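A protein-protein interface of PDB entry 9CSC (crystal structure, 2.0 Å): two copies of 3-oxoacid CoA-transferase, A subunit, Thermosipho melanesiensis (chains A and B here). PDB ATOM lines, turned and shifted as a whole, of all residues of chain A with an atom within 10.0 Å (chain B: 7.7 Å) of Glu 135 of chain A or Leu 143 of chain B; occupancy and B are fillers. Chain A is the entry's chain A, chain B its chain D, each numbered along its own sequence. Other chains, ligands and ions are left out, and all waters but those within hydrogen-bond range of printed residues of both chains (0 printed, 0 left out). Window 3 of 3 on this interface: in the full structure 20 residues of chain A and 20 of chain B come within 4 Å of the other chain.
The backbone NH (N) of Leu 116 of chain A lies within hydrogen-bond range of the backbone carbonyl oxygen (O) of Gly 114 of chain B (2.7 Å).
N of Leu 116 of chain B lies within hydrogen-bond range of O of Gly 114 of chain A (3.0 Å).
The backbone carbonyl oxygen (O) of Leu 116 of chain A sits at hydrogen-bond distance from the backbone NH (N) of Gly 113 of chain B, at 2.8 Å.
N of Leu 112 of chain B is in hydrogen-bond range of O of Ala 107 of chain B (3.0 Å).
O of Ile 115 of chain B lies within hydrogen-bond range of N of Glu 142 of chain B, at 2.9 Å.
The backbone NH of Ile 132 of chain A sits at hydrogen-bond distance from the backbone carbonyl oxygen of Tyr 139 of chain A (2.9 Å).
N of Leu 141 of chain B sits at hydrogen-bond distance from O of Lys 130 of chain B.
The guanidinium group (NE) of Arg 104 of chain B lies within hydrogen-bond range of the backbone carbonyl oxygen (O) of Leu 143 of chain B, at 2.7 Å.
Gly 114 of chain A touches Ile 115 of chain B.
CD2 of Leu 112 of chain B touches CD1 of Ile 115 of chain A, 3.5 Å away.
CA of Ile 115 of chain A touches O of Gly 114 of chain B (3.5 Å).
Leu 112 of chain B touches Leu 116 of chain A.
Leu 116 of chain A touches Leu 141 of chain B (CD2 to CD1, 3.8 Å).
Val 134 of chain A touches Gly 113 of chain B (CG2 to O, 3.9 Å).
Leu 143 of chain B touches Val 134 of chain A (CD2 to CG1, 3.3 Å).
Leu 143 of chain B touches Glu 135 of chain A.
CA of Gly 113 of chain B touches CE1 of Tyr 139 of chain A, 3.4 Å away.
Printed residues of chain B within 4 Å of Ile 115 of chain A: Leu 112 (3.5 Å) and Gly 114 (3.5 Å).
Glu 135 of chain A touches just one residue of chain B: Leu 143 (3.96 Å).
No residue of chain A comes within 4 Å of Arg 104 of chain B.
Of the printed residues of chain A, Leu 141 of chain B touches Leu 116 (3.8 Å).
Leu 143 of chain B touches two residues of chain A.
No residue of chain A comes within 4 Å of Pro 144 of chain B.
The nearest residue of chain B that does not touch Glu 135 of chain A is Pro 144 of chain B (5.5 Å).
The nearest printed residue of chain B that does not touch Tyr 139 of chain A is Leu 112 of chain B (4.4 Å).
Hydrophobic or aromatic side chains of chain A within 4 Å of the printed part of chain B: Ile 115, Leu 116, Val 134 and Tyr 139.
Along chain A the printed residues that touch a printed residue of chain B span positions 114 to 139.
Of the 22 printed residues of chain B, 7 touch a printed residue of chain A.
Printed residues of chain B that touch a printed residue of chain A: Leu 112, Gly 113, Gly 114, Ile 115, Leu 116, Leu 141 and Leu 143.
Hydrophobic or aromatic side chains of chain B within 4 Å of the printed part of chain A: Leu 112, Leu 116, Leu 141 and Leu 143.
Among the printed residues, no Asp or Glu carboxylate lies within 4 Å of a Lys or Arg side-chain nitrogen of the other chain.
Gly 114 of chain A touches Ile 115 of chain B, and with the chains exchanged Ile 115 of chain A touches Gly 114 of chain B.
Gly 114 of chain A touches Leu 116 of chain B, and with the chains exchanged Leu 116 of chain A touches Gly 114 of chain B.
3 positions are printed for both chains.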
ATOM      1  N   GLY A 114       6.638  -8.757  -1.628  1.00  0.00           N
ATOM      2  CA  GLY A 114       7.361  -9.947  -2.030  1.00  0.00           C
ATOM      3  C   GLY A 114       7.079 -10.290  -3.477  1.00  0.00           C
ATOM      4  O   GLY A 114       6.171  -9.737  -4.118  1.00  0.00           O
ATOM      5  N   ILE A 115       7.922 -11.181  -4.003  1.00  0.00           N
ATOM      6  CA  ILE A 115       7.748 -11.698  -5.356  1.00  0.00           C
ATOM      7  C   ILE A 115       7.972 -13.202  -5.303  1.00  0.00           C
ATOM      8  O   ILE A 115       8.763 -13.707  -4.499  1.00  0.00           O
ATOM      9  CB  ILE A 115       8.694 -11.038  -6.388  1.00  0.00           C
ATOM     10  CG1 ILE A 115      10.145 -11.343  -6.041  1.00  0.00           C
ATOM     11  CG2 ILE A 115       8.563  -9.487  -6.381  1.00  0.00           C
ATOM     12  CD1 ILE A 115      10.912 -11.853  -7.151  1.00  0.00           C
ATOM     13  N   LEU A 116       7.273 -13.912  -6.185  1.00  0.00           N
ATOM     14  CA  LEU A 116       7.442 -15.353  -6.363  1.00  0.00           C
ATOM     15  C   LEU A 116       8.427 -15.591  -7.484  1.00  0.00           C
ATOM     16  O   LEU A 116       8.148 -15.207  -8.620  1.00  0.00           O
ATOM     17  CB  LEU A 116       6.119 -16.031  -6.739  1.00  0.00           C
ATOM     18  CG  LEU A 116       5.231 -16.457  -5.576  1.00  0.00           C
ATOM     19  CD1 LEU A 116       4.945 -15.235  -4.662  1.00  0.00           C
ATOM     20  CD2 LEU A 116       3.882 -17.106  -6.031  1.00  0.00           C
ATOM     21  N   ILE A 132       5.418 -21.650  -2.825  1.00  0.00           N
ATOM     22  CA  ILE A 132       4.056 -21.382  -3.256  1.00  0.00           C
ATOM     23  C   ILE A 132       3.870 -22.017  -4.619  1.00  0.00           C
ATOM     24  O   ILE A 132       4.668 -21.777  -5.535  1.00  0.00           O
ATOM     25  CB  ILE A 132       3.760 -19.869  -3.276  1.00  0.00           C
ATOM     26  CG1 ILE A 132       4.140 -19.296  -1.903  1.00  0.00           C
ATOM     27  CG2 ILE A 132       2.360 -19.624  -3.620  1.00  0.00           C
ATOM     28  CD1 ILE A 132       3.455 -17.996  -1.474  1.00  0.00           C
ATOM     29  N   GLU A 133       2.815 -22.827  -4.749  1.00  0.00           N
ATOM     30  CA  GLU A 133       2.470 -23.437  -6.016  1.00  0.00           C
ATOM     31  C   GLU A 133       1.431 -22.575  -6.710  1.00  0.00           C
ATOM     32  O   GLU A 133       0.426 -22.187  -6.107  1.00  0.00           O
ATOM     33  CB  GLU A 133       1.978 -24.871  -5.825  1.00  0.00           C
ATOM     34  CG  GLU A 133       2.337 -25.717  -7.030  1.00  0.00           C
ATOM     35  CD  GLU A 133       2.484 -27.174  -6.668  1.00  0.00           C
ATOM     36  OE1 GLU A 133       3.102 -27.936  -7.416  1.00  0.00           O
ATOM     37  OE2 GLU A 133       2.031 -27.584  -5.601  1.00  0.00           O
ATOM     38  N   VAL A 134       1.704 -22.251  -7.967  1.00  0.00           N
ATOM     39  CA  VAL A 134       0.771 -21.523  -8.813  1.00  0.00           C
ATOM     40  C   VAL A 134       0.601 -22.374 -10.056  1.00  0.00           C
ATOM     41  O   VAL A 134       1.599 -22.731 -10.703  1.00  0.00           O
ATOM     42  CB  VAL A 134       1.284 -20.116  -9.182  1.00  0.00           C
ATOM     43  CG1 VAL A 134       0.255 -19.358 -10.010  1.00  0.00           C
ATOM     44  CG2 VAL A 134       1.610 -19.351  -7.946  1.00  0.00           C
ATOM     45  N   GLU A 135      -0.648 -22.729 -10.374  1.00  0.00           N
ATOM     46  CA  GLU A 135      -0.930 -23.515 -11.574  1.00  0.00           C
ATOM     47  C   GLU A 135       0.060 -24.678 -11.685  1.00  0.00           C
ATOM     48  O   GLU A 135       0.694 -24.913 -12.726  1.00  0.00           O
ATOM     49  CB  GLU A 135      -0.903 -22.608 -12.807  1.00  0.00           C
ATOM     50  CG  GLU A 135      -2.114 -21.626 -12.850  1.00  0.00           C
ATOM     51  CD  GLU A 135      -1.752 -20.162 -13.139  1.00  0.00           C
ATOM     52  OE1 GLU A 135      -0.718 -19.909 -13.787  1.00  0.00           O
ATOM     53  OE2 GLU A 135      -2.524 -19.243 -12.741  1.00  0.00           O
ATOM     54  N   GLY A 136       0.241 -25.359 -10.554  1.00  0.00           N
ATOM     55  CA  GLY A 136       1.029 -26.573 -10.534  1.00  0.00           C
ATOM     56  C   GLY A 136       2.515 -26.413 -10.713  1.00  0.00           C
ATOM     57  O   GLY A 136       3.183 -27.390 -11.064  1.00  0.00           O
ATOM     58  N   LYS A 137       3.061 -25.205 -10.471  1.00  0.00           N
ATOM     59  CA  LYS A 137       4.502 -24.983 -10.437  1.00  0.00           C
ATOM     60  C   LYS A 137       4.885 -24.338  -9.131  1.00  0.00           C
ATOM     61  O   LYS A 137       4.107 -23.556  -8.557  1.00  0.00           O
ATOM     62  CB  LYS A 137       4.990 -24.098 -11.614  1.00  0.00           C
ATOM     63  CG  LYS A 137       6.538 -23.981 -11.673  1.00  0.00           C
ATOM     64  CD  LYS A 137       7.023 -23.616 -13.091  1.00  0.00           C
ATOM     65  CE  LYS A 137       8.284 -22.776 -13.188  1.00  0.00           C
ATOM     66  NZ  LYS A 137       9.557 -23.636 -13.188  1.00  0.00           N
ATOM     67  N   LYS A 138       6.096 -24.666  -8.700  1.00  0.00           N
ATOM     68  CA  LYS A 138       6.627 -24.198  -7.433  1.00  0.00           C
ATOM     69  C   LYS A 138       7.438 -22.917  -7.623  1.00  0.00           C
ATOM     70  O   LYS A 138       8.179 -22.792  -8.597  1.00  0.00           O
ATOM     71  CB  LYS A 138       7.516 -25.273  -6.811  1.00  0.00           C
ATOM     72  CG  LYS A 138       6.747 -26.428  -6.227  1.00  0.00           C
ATOM     73  CD  LYS A 138       7.691 -27.509  -5.726  1.00  0.00           C
ATOM     74  CE  LYS A 138       7.111 -28.906  -5.775  1.00  0.00           C
ATOM     75  NZ  LYS A 138       5.715 -28.898  -5.226  1.00  0.00           N
ATOM     76  N   TYR A 139       7.306 -21.974  -6.674  1.00  0.00           N
ATOM     77  CA  TYR A 139       8.101 -20.749  -6.614  1.00  0.00           C
ATOM     78  C   TYR A 139       8.529 -20.523  -5.177  1.00  0.00           C
ATOM     79  O   TYR A 139       7.785 -20.848  -4.247  1.00  0.00           O
ATOM     80  CB  TYR A 139       7.272 -19.582  -7.100  1.00  0.00           C
ATOM     81  CG  TYR A 139       6.747 -19.742  -8.527  1.00  0.00           C
ATOM     82  CD1 TYR A 139       7.504 -19.342  -9.617  1.00  0.00           C
ATOM     83  CD2 TYR A 139       5.479 -20.277  -8.769  1.00  0.00           C
ATOM     84  CE1 TYR A 139       7.005 -19.428 -10.924  1.00  0.00           C
ATOM     85  CE2 TYR A 139       4.980 -20.408 -10.072  1.00  0.00           C
ATOM     86  CZ  TYR A 139       5.749 -19.980 -11.143  1.00  0.00           C
ATOM     87  OH  TYR A 139       5.243 -20.090 -12.413  1.00  0.00           O
ATOM     88  N   THR B 100      -1.689  -2.874  -9.903  1.00  0.00           N
ATOM     89  CA  THR B 100      -1.704  -4.320  -9.921  1.00  0.00           C
ATOM     90  C   THR B 100      -1.690  -4.857 -11.353  1.00  0.00           C
ATOM     91  O   THR B 100      -0.980  -5.821 -11.650  1.00  0.00           O
ATOM     92  CB  THR B 100      -2.947  -4.791  -9.153  1.00  0.00           C
ATOM     93  OG1 THR B 100      -2.864  -4.290  -7.805  1.00  0.00           O
ATOM     94  CG2 THR B 100      -3.081  -6.319  -9.219  1.00  0.00           C
ATOM     95  N   LEU B 101      -2.433  -4.227 -12.260  1.00  0.00           N
ATOM     96  CA  LEU B 101      -2.377  -4.668 -13.661  1.00  0.00           C
ATOM     97  C   LEU B 101      -0.967  -4.541 -14.258  1.00  0.00           C
ATOM     98  O   LEU B 101      -0.489  -5.437 -14.958  1.00  0.00           O
ATOM     99  CB  LEU B 101      -3.355  -3.850 -14.494  1.00  0.00           C
ATOM    100  CG  LEU B 101      -3.670  -4.341 -15.899  1.00  0.00           C
ATOM    101  CD1 LEU B 101      -4.287  -5.764 -15.932  1.00  0.00           C
ATOM    102  CD2 LEU B 101      -4.615  -3.346 -16.613  1.00  0.00           C
ATOM    103  N   GLU B 103       1.901  -4.662 -12.658  1.00  0.00           N
ATOM    104  CA  GLU B 103       2.808  -5.634 -12.061  1.00  0.00           C
ATOM    105  C   GLU B 103       2.490  -7.068 -12.504  1.00  0.00           C
ATOM    106  O   GLU B 103       3.402  -7.883 -12.676  1.00  0.00           O
ATOM    107  CB  GLU B 103       2.762  -5.535 -10.522  1.00  0.00           C
ATOM    108  CG  GLU B 103       3.573  -4.375  -9.896  1.00  0.00           C
ATOM    109  CD  GLU B 103       4.982  -4.169 -10.487  1.00  0.00           C
ATOM    110  OE1 GLU B 103       5.815  -5.094 -10.417  1.00  0.00           O
ATOM    111  OE2 GLU B 103       5.230  -3.057 -11.050  1.00  0.00           O
ATOM    112  N   ARG B 104       1.217  -7.406 -12.651  1.00  0.00           N
ATOM    113  CA  ARG B 104       0.866  -8.765 -13.065  1.00  0.00           C
ATOM    114  C   ARG B 104       1.293  -9.035 -14.506  1.00  0.00           C
ATOM    115  O   ARG B 104       1.731 -10.152 -14.853  1.00  0.00           O
ATOM    116  CB  ARG B 104      -0.653  -8.987 -12.903  1.00  0.00           C
ATOM    117  CG  ARG B 104      -1.204  -9.053 -11.491  1.00  0.00           C
ATOM    118  CD  ARG B 104      -2.717  -9.193 -11.482  1.00  0.00           C
ATOM    119  NE  ARG B 104      -3.100 -10.474 -12.083  1.00  0.00           N
ATOM    120  CZ  ARG B 104      -4.333 -10.823 -12.407  1.00  0.00           C
ATOM    121  NH1 ARG B 104      -5.359 -10.013 -12.203  1.00  0.00           N
ATOM    122  NH2 ARG B 104      -4.547 -12.030 -12.921  1.00  0.00           N
ATOM    123  N   ILE B 105       1.198  -8.013 -15.360  1.00  0.00           N
ATOM    124  CA  ILE B 105       1.656  -8.177 -16.735  1.00  0.00           C
ATOM    125  C   ILE B 105       3.170  -8.255 -16.750  1.00  0.00           C
ATOM    126  O   ILE B 105       3.764  -9.123 -17.397  1.00  0.00           O
ATOM    127  CB  ILE B 105       1.115  -7.043 -17.628  1.00  0.00           C
ATOM    128  CG1 ILE B 105      -0.379  -7.177 -17.880  1.00  0.00           C
ATOM    129  CG2 ILE B 105       1.844  -7.027 -18.921  1.00  0.00           C
ATOM    130  CD1 ILE B 105      -0.985  -5.945 -18.466  1.00  0.00           C
ATOM    131  N   ALA B 107       4.968  -9.318 -14.340  1.00  0.00           N
ATOM    132  CA  ALA B 107       5.421 -10.583 -13.778  1.00  0.00           C
ATOM    133  C   ALA B 107       5.547 -11.640 -14.871  1.00  0.00           C
ATOM    134  O   ALA B 107       6.523 -12.386 -14.912  1.00  0.00           O
ATOM    135  CB  ALA B 107       4.451 -11.049 -12.703  1.00  0.00           C
ATOM    136  N   ALA B 108       4.566 -11.710 -15.763  1.00  0.00           N
ATOM    137  CA  ALA B 108       4.612 -12.702 -16.840  1.00  0.00           C
ATOM    138  C   ALA B 108       5.790 -12.438 -17.785  1.00  0.00           C
ATOM    139  O   ALA B 108       6.445 -13.373 -18.271  1.00  0.00           O
ATOM    140  CB  ALA B 108       3.298 -12.668 -17.617  1.00  0.00           C
ATOM    141  N   LEU B 112       8.241 -14.089 -13.175  1.00  0.00           N
ATOM    142  CA  LEU B 112       7.832 -14.302 -11.792  1.00  0.00           C
ATOM    143  C   LEU B 112       6.540 -15.114 -11.771  1.00  0.00           C
ATOM    144  O   LEU B 112       5.711 -15.019 -12.681  1.00  0.00           O
ATOM    145  CB  LEU B 112       7.600 -12.975 -11.092  1.00  0.00           C
ATOM    146  CG  LEU B 112       8.810 -12.040 -11.153  1.00  0.00           C
ATOM    147  CD1 LEU B 112       8.438 -10.624 -10.618  1.00  0.00           C
ATOM    148  CD2 LEU B 112       9.896 -12.652 -10.387  1.00  0.00           C
ATOM    149  N   GLY B 113       6.378 -15.912 -10.718  1.00  0.00           N
ATOM    150  CA  GLY B 113       5.132 -16.605 -10.486  1.00  0.00           C
ATOM    151  C   GLY B 113       4.083 -15.737  -9.833  1.00  0.00           C
ATOM    152  O   GLY B 113       2.926 -16.139  -9.727  1.00  0.00           O
ATOM    153  N   GLY B 114       4.454 -14.550  -9.392  1.00  0.00           N
ATOM    154  CA  GLY B 114       3.493 -13.708  -8.717  1.00  0.00           C
ATOM    155  C   GLY B 114       4.164 -12.636  -7.891  1.00  0.00           C
ATOM    156  O   GLY B 114       5.380 -12.624  -7.701  1.00  0.00           O
ATOM    157  N   ILE B 115       3.330 -11.690  -7.443  1.00  0.00           N
ATOM    158  CA  ILE B 115       3.753 -10.558  -6.640  1.00  0.00           C
ATOM    159  C   ILE B 115       2.752 -10.392  -5.513  1.00  0.00           C
ATOM    160  O   ILE B 115       1.561 -10.660  -5.691  1.00  0.00           O
ATOM    161  CB  ILE B 115       3.793  -9.287  -7.478  1.00  0.00           C
ATOM    162  CG1 ILE B 115       2.433  -9.209  -8.127  1.00  0.00           C
ATOM    163  CG2 ILE B 115       4.850  -9.389  -8.553  1.00  0.00           C
ATOM    164  CD1 ILE B 115       1.965  -7.898  -8.474  1.00  0.00           C
ATOM    165  N   LEU B 116       3.218  -9.869  -4.378  1.00  0.00           N
ATOM    166  CA  LEU B 116       2.334  -9.499  -3.284  1.00  0.00           C
ATOM    167  C   LEU B 116       2.140  -7.995  -3.315  1.00  0.00           C
ATOM    168  O   LEU B 116       3.112  -7.247  -3.263  1.00  0.00           O
ATOM    169  CB  LEU B 116       2.889  -9.946  -1.936  1.00  0.00           C
ATOM    170  CG  LEU B 116       3.401 -11.384  -1.818  1.00  0.00           C
ATOM    171  CD1 LEU B 116       3.767 -11.733  -0.401  1.00  0.00           C
ATOM    172  CD2 LEU B 116       2.389 -12.348  -2.373  1.00  0.00           C
ATOM    173  N   ASP B 128     -11.714 -13.884  -3.665  1.00  0.00           N
ATOM    174  CA  ASP B 128     -11.097 -14.997  -4.383  1.00  0.00           C
ATOM    175  C   ASP B 128      -9.574 -14.906  -4.486  1.00  0.00           C
ATOM    176  O   ASP B 128      -8.962 -15.640  -5.281  1.00  0.00           O
ATOM    177  CB  ASP B 128     -11.646 -15.121  -5.810  1.00  0.00           C
ATOM    178  CG  ASP B 128     -13.031 -15.718  -5.864  1.00  0.00           C
ATOM    179  OD1 ASP B 128     -13.677 -15.878  -4.799  1.00  0.00           O
ATOM    180  OD2 ASP B 128     -13.472 -16.011  -6.997  1.00  0.00           O
ATOM    181  N   LYS B 129      -8.917 -14.052  -3.714  1.00  0.00           N
ATOM    182  CA  LYS B 129      -7.462 -14.005  -3.737  1.00  0.00           C
ATOM    183  C   LYS B 129      -6.853 -14.629  -2.487  1.00  0.00           C
ATOM    184  O   LYS B 129      -7.404 -14.499  -1.379  1.00  0.00           O
ATOM    185  CB  LYS B 129      -6.973 -12.555  -3.926  1.00  0.00           C
ATOM    186  CG  LYS B 129      -6.714 -12.229  -5.431  1.00  0.00           C
ATOM    187  CD  LYS B 129      -7.498 -11.002  -5.881  1.00  0.00           C
ATOM    188  CE  LYS B 129      -7.122 -10.598  -7.302  1.00  0.00           C
ATOM    189  NZ  LYS B 129      -7.815  -9.375  -7.742  1.00  0.00           N
ATOM    190  N   LYS B 130      -5.703 -15.297  -2.677  1.00  0.00           N
ATOM    191  CA  LYS B 130      -4.890 -15.705  -1.535  1.00  0.00           C
ATOM    192  C   LYS B 130      -4.341 -14.462  -0.822  1.00  0.00           C
ATOM    193  O   LYS B 130      -3.900 -13.492  -1.463  1.00  0.00           O
ATOM    194  CB  LYS B 130      -3.728 -16.590  -1.949  1.00  0.00           C
ATOM    195  CG  LYS B 130      -3.305 -17.569  -0.818  1.00  0.00           C
ATOM    196  CD  LYS B 130      -2.239 -18.578  -1.286  1.00  0.00           C
ATOM    197  CE  LYS B 130      -2.176 -19.899  -0.425  1.00  0.00           C
ATOM    198  NZ  LYS B 130      -2.279 -21.196  -1.323  1.00  0.00           N
ATOM    199  N   LEU B 140      -2.180  -9.083  -0.961  1.00  0.00           N
ATOM    200  CA  LEU B 140      -2.824 -10.013  -1.883  1.00  0.00           C
ATOM    201  C   LEU B 140      -1.771 -10.611  -2.806  1.00  0.00           C
ATOM    202  O   LEU B 140      -0.934  -9.878  -3.355  1.00  0.00           O
ATOM    203  CB  LEU B 140      -3.894  -9.314  -2.720  1.00  0.00           C
ATOM    204  CG  LEU B 140      -4.910  -8.443  -1.990  1.00  0.00           C
ATOM    205  CD1 LEU B 140      -5.894  -7.840  -3.010  1.00  0.00           C
ATOM    206  CD2 LEU B 140      -5.642  -9.246  -0.886  1.00  0.00           C
ATOM    207  N   LEU B 141      -1.850 -11.928  -3.026  1.00  0.00           N
ATOM    208  CA  LEU B 141      -1.066 -12.581  -4.063  1.00  0.00           C
ATOM    209  C   LEU B 141      -1.798 -12.328  -5.386  1.00  0.00           C
ATOM    210  O   LEU B 141      -3.001 -12.588  -5.508  1.00  0.00           O
ATOM    211  CB  LEU B 141      -0.888 -14.070  -3.749  1.00  0.00           C
ATOM    212  CG  LEU B 141      -0.291 -14.960  -4.847  1.00  0.00           C
ATOM    213  CD1 LEU B 141       1.142 -14.603  -5.183  1.00  0.00           C
ATOM    214  CD2 LEU B 141      -0.331 -16.459  -4.467  1.00  0.00           C
ATOM    215  N   GLU B 142      -1.111 -11.698  -6.333  1.00  0.00           N
ATOM    216  CA  GLU B 142      -1.688 -11.398  -7.634  1.00  0.00           C
ATOM    217  C   GLU B 142      -0.817 -12.074  -8.675  1.00  0.00           C
ATOM    218  O   GLU B 142       0.401 -12.135  -8.532  1.00  0.00           O
ATOM    219  CB  GLU B 142      -1.827  -9.895  -7.835  1.00  0.00           C
ATOM    220  CG  GLU B 142      -2.772  -9.250  -6.829  1.00  0.00           C
ATOM    221  CD  GLU B 142      -4.171  -9.091  -7.368  1.00  0.00           C
ATOM    222  OE1 GLU B 142      -4.472  -9.744  -8.375  1.00  0.00           O
ATOM    223  OE2 GLU B 142      -4.970  -8.300  -6.822  1.00  0.00           O
ATOM    224  N   LEU B 143      -1.456 -12.627  -9.687  1.00  0.00           N
ATOM    225  CA  LEU B 143      -0.824 -13.657 -10.489  1.00  0.00           C
ATOM    226  C   LEU B 143      -0.454 -13.133 -11.868  1.00  0.00           C
ATOM    227  O   LEU B 143      -1.081 -12.201 -12.354  1.00  0.00           O
ATOM    228  CB  LEU B 143      -1.807 -14.827 -10.587  1.00  0.00           C
ATOM    229  CG  LEU B 143      -1.885 -15.699  -9.318  1.00  0.00           C
ATOM    230  CD1 LEU B 143      -2.889 -16.842  -9.615  1.00  0.00           C
ATOM    231  CD2 LEU B 143      -0.572 -16.285  -8.964  1.00  0.00           C
ATOM    232  N   PRO B 144       0.537 -13.713 -12.536  1.00  0.00           N
ATOM    233  CA  PRO B 144       0.917 -13.193 -13.857  1.00  0.00           C
ATOM    234  C   PRO B 144      -0.226 -13.288 -14.862  1.00  0.00           C
ATOM    235  O   PRO B 144      -1.061 -14.190 -14.825  1.00  0.00           O
ATOM    236  CB  PRO B 144       2.096 -14.078 -14.277  1.00  0.00           C
ATOM    237  CG  PRO B 144       2.429 -14.933 -13.002  1.00  0.00           C
ATOM    238  CD  PRO B 144       1.214 -14.974 -12.192  1.00  0.00           C
ATOM    239  N   ILE B 145      -0.258 -12.310 -15.761  1.00  0.00           N
ATOM    240  CA  ILE B 145      -1.263 -12.210 -16.809  1.00  0.00           C
ATOM    241  C   ILE B 145      -0.583 -12.412 -18.156  1.00  0.00           C
ATOM    242  O   ILE B 145       0.197 -11.564 -18.606  1.00  0.00           O
ATOM    243  CB  ILE B 145      -1.969 -10.854 -16.783  1.00  0.00           C
ATOM    244  CG1 ILE B 145      -2.753 -10.655 -15.488  1.00  0.00           C
ATOM    245  CG2 ILE B 145      -2.819 -10.680 -18.071  1.00  0.00           C
ATOM    246  CD1 ILE B 145      -3.052  -9.154 -15.227  1.00  0.00           C
ATOM    247  N   HIS B 146      -0.881 -13.526 -18.804  1.00  0.00           N
ATOM    248  CA  HIS B 146      -0.271 -13.872 -20.078  1.00  0.00           C
ATOM    249  C   HIS B 146      -1.192 -13.536 -21.257  1.00  0.00           C
ATOM    250  O   HIS B 146      -2.394 -13.271 -21.093  1.00  0.00           O
ATOM    251  CB  HIS B 146       0.074 -15.351 -20.105  1.00  0.00           C
ATOM    252  CG  HIS B 146       1.307 -15.719 -19.354  1.00  0.00           C
ATOM    253  ND1 HIS B 146       1.275 -16.225 -18.072  1.00  0.00           N
ATOM    254  CD2 HIS B 146       2.610 -15.719 -19.720  1.00  0.00           C
ATOM    255  CE1 HIS B 146       2.501 -16.532 -17.686  1.00  0.00           C
ATOM    256  NE2 HIS B 146       3.332 -16.223 -18.667  1.00  0.00           N
